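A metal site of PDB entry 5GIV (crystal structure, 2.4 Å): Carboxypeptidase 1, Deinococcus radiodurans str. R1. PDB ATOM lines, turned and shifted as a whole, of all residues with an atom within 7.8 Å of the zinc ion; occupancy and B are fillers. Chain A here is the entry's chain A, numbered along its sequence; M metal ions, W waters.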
ATOM      1  N   PRO A 236      18.967   2.604 -10.897  1.00  0.00           N
ATOM      2  CA  PRO A 236      18.610   1.204 -10.642  1.00  0.00           C
ATOM      3  C   PRO A 236      19.113   0.287 -11.752  1.00  0.00           C
ATOM      4  O   PRO A 236      19.066   0.639 -12.937  1.00  0.00           O
ATOM      5  CB  PRO A 236      17.079   1.235 -10.601  1.00  0.00           C
ATOM      6  CG  PRO A 236      16.732   2.627 -10.266  1.00  0.00           C
ATOM      7  CD  PRO A 236      17.793   3.487 -10.896  1.00  0.00           C
ATOM      8  N   PHE A 237      19.577  -0.901 -11.367  1.00  0.00           N
ATOM      9  CA  PHE A 237      20.001  -1.903 -12.343  1.00  0.00           C
ATOM     10  C   PHE A 237      19.985  -3.271 -11.687  1.00  0.00           C
ATOM     11  O   PHE A 237      19.790  -3.403 -10.477  1.00  0.00           O
ATOM     12  CB  PHE A 237      21.384  -1.577 -12.914  1.00  0.00           C
ATOM     13  CG  PHE A 237      22.481  -1.586 -11.891  1.00  0.00           C
ATOM     14  CD1 PHE A 237      22.801  -0.433 -11.193  1.00  0.00           C
ATOM     15  CD2 PHE A 237      23.210  -2.744 -11.631  1.00  0.00           C
ATOM     16  CE1 PHE A 237      23.826  -0.433 -10.253  1.00  0.00           C
ATOM     17  CE2 PHE A 237      24.216  -2.745 -10.689  1.00  0.00           C
ATOM     18  CZ  PHE A 237      24.534  -1.585  -9.997  1.00  0.00           C
ATOM     19  N   MET A 238      20.178  -4.295 -12.507  1.00  0.00           N
ATOM     20  CA  MET A 238      20.307  -5.676 -12.063  1.00  0.00           C
ATOM     21  C   MET A 238      21.641  -6.217 -12.562  1.00  0.00           C
ATOM     22  O   MET A 238      22.047  -5.916 -13.694  1.00  0.00           O
ATOM     23  CB  MET A 238      19.136  -6.532 -12.561  1.00  0.00           C
ATOM     24  CG  MET A 238      19.165  -8.014 -12.167  1.00  0.00           C
ATOM     25  SD  MET A 238      19.998  -9.077 -13.372  1.00  0.00           S
ATOM     26  CE  MET A 238      18.813  -9.024 -14.681  1.00  0.00           C
ATOM     27  N   HIS A 266      10.613  -3.380 -11.034  1.00  0.00           N
ATOM     28  CA  HIS A 266      11.197  -3.561 -12.357  1.00  0.00           C
ATOM     29  C   HIS A 266      12.468  -4.394 -12.288  1.00  0.00           C
ATOM     30  O   HIS A 266      12.591  -5.434 -12.943  1.00  0.00           O
ATOM     31  CB  HIS A 266      11.469  -2.195 -12.989  1.00  0.00           C
ATOM     32  CG  HIS A 266      12.039  -2.259 -14.359  1.00  0.00           C
ATOM     33  ND1 HIS A 266      11.288  -2.039 -15.499  1.00  0.00           N
ATOM     34  CD2 HIS A 266      13.303  -2.517 -14.795  1.00  0.00           C
ATOM     35  CE1 HIS A 266      12.061  -2.150 -16.562  1.00  0.00           C
ATOM     36  NE2 HIS A 266      13.289  -2.441 -16.167  1.00  0.00           N
ATOM     37  N   GLU A 267      13.458  -3.951 -11.493  1.00  0.00           N
ATOM     38  CA  GLU A 267      14.724  -4.679 -11.410  1.00  0.00           C
ATOM     39  C   GLU A 267      14.562  -6.073 -10.801  1.00  0.00           C
ATOM     40  O   GLU A 267      15.255  -7.016 -11.208  1.00  0.00           O
ATOM     41  CB  GLU A 267      15.765  -3.887 -10.607  1.00  0.00           C
ATOM     42  CG  GLU A 267      16.165  -2.526 -11.191  1.00  0.00           C
ATOM     43  CD  GLU A 267      16.680  -2.617 -12.613  1.00  0.00           C
ATOM     44  OE1 GLU A 267      17.281  -3.645 -12.993  1.00  0.00           O
ATOM     45  OE2 GLU A 267      16.488  -1.637 -13.354  1.00  0.00           O
ATOM     46  N   HIS A 270      13.751  -8.340 -13.644  1.00  0.00           N
ATOM     47  CA  HIS A 270      14.996  -8.786 -14.247  1.00  0.00           C
ATOM     48  C   HIS A 270      15.620  -9.911 -13.436  1.00  0.00           C
ATOM     49  O   HIS A 270      16.058 -10.922 -13.979  1.00  0.00           O
ATOM     50  CB  HIS A 270      15.978  -7.617 -14.383  1.00  0.00           C
ATOM     51  CG  HIS A 270      15.680  -6.679 -15.506  1.00  0.00           C
ATOM     52  ND1 HIS A 270      15.503  -7.107 -16.811  1.00  0.00           N
ATOM     53  CD2 HIS A 270      15.523  -5.330 -15.534  1.00  0.00           C
ATOM     54  CE1 HIS A 270      15.261  -6.062 -17.591  1.00  0.00           C
ATOM     55  NE2 HIS A 270      15.269  -4.980 -16.836  1.00  0.00           N
ATOM     56  N   ALA A 292      17.635  -9.046 -24.975  1.00  0.00           N
ATOM     57  CA  ALA A 292      17.221  -7.831 -24.293  1.00  0.00           C
ATOM     58  C   ALA A 292      15.715  -7.754 -24.188  1.00  0.00           C
ATOM     59  O   ALA A 292      15.168  -7.389 -23.137  1.00  0.00           O
ATOM     60  CB  ALA A 292      17.773  -6.601 -25.013  1.00  0.00           C
ATOM     61  N   HIS A 295      14.352 -10.192 -21.656  1.00  0.00           N
ATOM     62  CA  HIS A 295      14.693  -9.731 -20.313  1.00  0.00           C
ATOM     63  C   HIS A 295      13.781  -8.604 -19.866  1.00  0.00           C
ATOM     64  O   HIS A 295      13.150  -8.670 -18.803  1.00  0.00           O
ATOM     65  CB  HIS A 295      16.158  -9.297 -20.251  1.00  0.00           C
ATOM     66  CG  HIS A 295      16.903  -9.915 -19.108  1.00  0.00           C
ATOM     67  ND1 HIS A 295      16.558  -9.686 -17.792  1.00  0.00           N
ATOM     68  CD2 HIS A 295      17.928 -10.792 -19.090  1.00  0.00           C
ATOM     69  CE1 HIS A 295      17.355 -10.389 -17.004  1.00  0.00           C
ATOM     70  NE2 HIS A 295      18.200 -11.065 -17.763  1.00  0.00           N
ATOM     71  N   GLU A 296      13.666  -7.557 -20.683  1.00  0.00           N
ATOM     72  CA  GLU A 296      12.790  -6.434 -20.355  1.00  0.00           C
ATOM     73  C   GLU A 296      11.327  -6.840 -20.308  1.00  0.00           C
ATOM     74  O   GLU A 296      10.519  -6.123 -19.708  1.00  0.00           O
ATOM     75  CB  GLU A 296      12.991  -5.302 -21.351  1.00  0.00           C
ATOM     76  CG  GLU A 296      12.273  -4.017 -20.975  1.00  0.00           C
ATOM     77  CD  GLU A 296      12.971  -3.266 -19.859  1.00  0.00           C
ATOM     78  OE1 GLU A 296      12.660  -2.074 -19.670  1.00  0.00           O
ATOM     79  OE2 GLU A 296      13.822  -3.861 -19.157  1.00  0.00           O
ATOM     80  N   SER A 297      10.950  -7.942 -20.953  1.00  0.00           N
ATOM     81  CA  SER A 297       9.579  -8.412 -20.843  1.00  0.00           C
ATOM     82  C   SER A 297       9.267  -8.815 -19.414  1.00  0.00           C
ATOM     83  O   SER A 297       8.112  -8.700 -18.980  1.00  0.00           O
ATOM     84  CB  SER A 297       9.336  -9.615 -21.768  1.00  0.00           C
ATOM     85  OG  SER A 297       9.863 -10.807 -21.199  1.00  0.00           O
ATOM     86  N   GLN A 298      10.273  -9.268 -18.687  1.00  0.00           N
ATOM     87  CA  GLN A 298      10.057  -9.760 -17.334  1.00  0.00           C
ATOM     88  C   GLN A 298      10.086  -8.625 -16.307  1.00  0.00           C
ATOM     89  O   GLN A 298       9.283  -8.613 -15.367  1.00  0.00           O
ATOM     90  CB  GLN A 298      11.108 -10.819 -17.037  1.00  0.00           C
ATOM     91  CG  GLN A 298      10.914 -12.013 -17.961  1.00  0.00           C
ATOM     92  CD  GLN A 298       9.455 -12.470 -17.989  1.00  0.00           C
ATOM     93  OE1 GLN A 298       8.900 -12.857 -16.957  1.00  0.00           O
ATOM     94  NE2 GLN A 298       8.832 -12.433 -19.164  1.00  0.00           N
ATOM     95  N   SER A 299      10.984  -7.650 -16.480  1.00  0.00           N
ATOM     96  CA  SER A 299      10.907  -6.472 -15.630  1.00  0.00           C
ATOM     97  C   SER A 299       9.568  -5.769 -15.820  1.00  0.00           C
ATOM     98  O   SER A 299       8.938  -5.361 -14.841  1.00  0.00           O
ATOM     99  CB  SER A 299      12.085  -5.545 -15.928  1.00  0.00           C
ATOM    100  OG  SER A 299      12.191  -5.292 -17.304  1.00  0.00           O
ATOM    101  N   ARG A 300       9.113  -5.640 -17.060  1.00  0.00           N
ATOM    102  CA  ARG A 300       7.857  -4.948 -17.326  1.00  0.00           C
ATOM    103  C   ARG A 300       6.661  -5.774 -16.876  1.00  0.00           C
ATOM    104  O   ARG A 300       5.623  -5.209 -16.499  1.00  0.00           O
ATOM    105  CB  ARG A 300       7.762  -4.613 -18.813  1.00  0.00           C
ATOM    106  CG  ARG A 300       8.754  -3.537 -19.242  1.00  0.00           C
ATOM    107  CD  ARG A 300       8.554  -2.256 -18.434  1.00  0.00           C
ATOM    108  NE  ARG A 300       9.182  -1.120 -19.077  1.00  0.00           N
ATOM    109  CZ  ARG A 300       9.097   0.138 -18.656  1.00  0.00           C
ATOM    110  NH1 ARG A 300       8.387   0.428 -17.567  1.00  0.00           N
ATOM    111  NH2 ARG A 300       9.701   1.112 -19.327  1.00  0.00           N
ATOM    112  N   GLU A 303       6.657  -5.271 -13.092  1.00  0.00           N
ATOM    113  CA  GLU A 303       6.464  -3.873 -12.734  1.00  0.00           C
ATOM    114  C   GLU A 303       5.081  -3.383 -13.146  1.00  0.00           C
ATOM    115  O   GLU A 303       4.335  -2.871 -12.317  1.00  0.00           O
ATOM    116  CB  GLU A 303       7.551  -3.003 -13.389  1.00  0.00           C
ATOM    117  CG  GLU A 303       7.342  -1.494 -13.193  1.00  0.00           C
ATOM    118  CD  GLU A 303       8.047  -0.616 -14.241  1.00  0.00           C
ATOM    119  OE1 GLU A 303       7.920   0.615 -14.166  1.00  0.00           O
ATOM    120  OE2 GLU A 303       8.735  -1.161 -15.143  1.00  0.00           O
ATOM    121  N   ARG A 349      12.862   9.490 -20.726  1.00  0.00           N
ATOM    122  CA  ARG A 349      12.428   8.195 -21.197  1.00  0.00           C
ATOM    123  C   ARG A 349      12.167   7.239 -20.033  1.00  0.00           C
ATOM    124  O   ARG A 349      11.133   6.572 -19.986  1.00  0.00           O
ATOM    125  CB  ARG A 349      13.455   7.601 -22.161  1.00  0.00           C
ATOM    126  CG  ARG A 349      13.160   6.166 -22.559  1.00  0.00           C
ATOM    127  CD  ARG A 349      14.295   5.574 -23.385  1.00  0.00           C
ATOM    128  NE  ARG A 349      15.543   5.671 -22.639  1.00  0.00           N
ATOM    129  CZ  ARG A 349      15.959   4.758 -21.773  1.00  0.00           C
ATOM    130  NH1 ARG A 349      15.225   3.667 -21.550  1.00  0.00           N
ATOM    131  NH2 ARG A 349      17.108   4.935 -21.130  1.00  0.00           N
ATOM    132  N   TYR A 357       5.631   5.801 -23.452  1.00  0.00           N
ATOM    133  CA  TYR A 357       7.024   5.369 -23.344  1.00  0.00           C
ATOM    134  C   TYR A 357       7.629   5.079 -24.705  1.00  0.00           C
ATOM    135  O   TYR A 357       8.745   5.521 -25.013  1.00  0.00           O
ATOM    136  CB  TYR A 357       7.130   4.125 -22.446  1.00  0.00           C
ATOM    137  CG  TYR A 357       8.564   3.648 -22.275  1.00  0.00           C
ATOM    138  CD1 TYR A 357       9.141   2.757 -23.185  1.00  0.00           C
ATOM    139  CD2 TYR A 357       9.341   4.118 -21.237  1.00  0.00           C
ATOM    140  CE1 TYR A 357      10.458   2.339 -23.031  1.00  0.00           C
ATOM    141  CE2 TYR A 357      10.658   3.707 -21.075  1.00  0.00           C
ATOM    142  CZ  TYR A 357      11.206   2.820 -21.974  1.00  0.00           C
ATOM    143  OH  TYR A 357      12.494   2.414 -21.802  1.00  0.00           O
ATOM    144  N   TYR A 422      13.900  -2.137 -25.234  1.00  0.00           N
ATOM    145  CA  TYR A 422      12.954  -1.661 -24.239  1.00  0.00           C
ATOM    146  C   TYR A 422      11.519  -1.808 -24.729  1.00  0.00           C
ATOM    147  O   TYR A 422      10.628  -2.213 -23.976  1.00  0.00           O
ATOM    148  CB  TYR A 422      13.244  -0.203 -23.875  1.00  0.00           C
ATOM    149  CG  TYR A 422      14.615   0.032 -23.285  1.00  0.00           C
ATOM    150  CD1 TYR A 422      14.952  -0.451 -22.031  1.00  0.00           C
ATOM    151  CD2 TYR A 422      15.565   0.770 -23.974  1.00  0.00           C
ATOM    152  CE1 TYR A 422      16.198  -0.234 -21.484  1.00  0.00           C
ATOM    153  CE2 TYR A 422      16.818   1.003 -23.441  1.00  0.00           C
ATOM    154  CZ  TYR A 422      17.127   0.489 -22.185  1.00  0.00           C
ATOM    155  OH  TYR A 422      18.382   0.715 -21.646  1.00  0.00           O
HETATM  156 ZN    ZN M   1      14.974  -2.935 -17.559  1.00  0.00          ZN
HETATM  157  O   HOH W   1      17.276  -3.186 -18.327  1.00  0.00           O
HETATM  158  O   HOH W   2      16.716  -2.027 -16.173  1.00  0.00           O
HETATM  159  O   HOH W   3      14.552  -1.020 -18.145  1.00  0.00           O
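O of Glu 296 lies within hydrogen-bond range of OG of Ser 299 (3.0 Å). The side-chain carboxylate (OE1) of Glu 296 is in salt-bridge range of the guanidinium group (NE) of Arg 300, at 3.7 Å. NE2 of His 270 lies close to OG of Ser 299 (3.1 Å). A ring nitrogen (ND1) of His 270 is in hydrogen-bond range of a ring nitrogen (ND1) of His 295 (3.0 Å). OG of Ser 299 sits close to NE2 of His 266 (3.3 Å). A ring nitrogen (ND1) of His 266 sits at hydrogen-bond distance from the side-chain carboxylate (OE2) of Glu 303 (2.7 Å).
Merely in contact with the zinc ion: Ser 299 (3.7 Å).
Water W3 binds the zinc ion (2.0 Å). OE2 of Glu 296 is bound to the zinc ion (2.2 Å). A ring nitrogen (NE2) of His 270 binds the zinc ion, at 2.2 Å. NE2 of His 266 is bound to the zinc ion, 2.2 Å away. The zinc ion is bound by water W2 (2.4 Å). Water W1 is bound to the zinc ion. The zinc ion has six donor atoms within binding distance.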
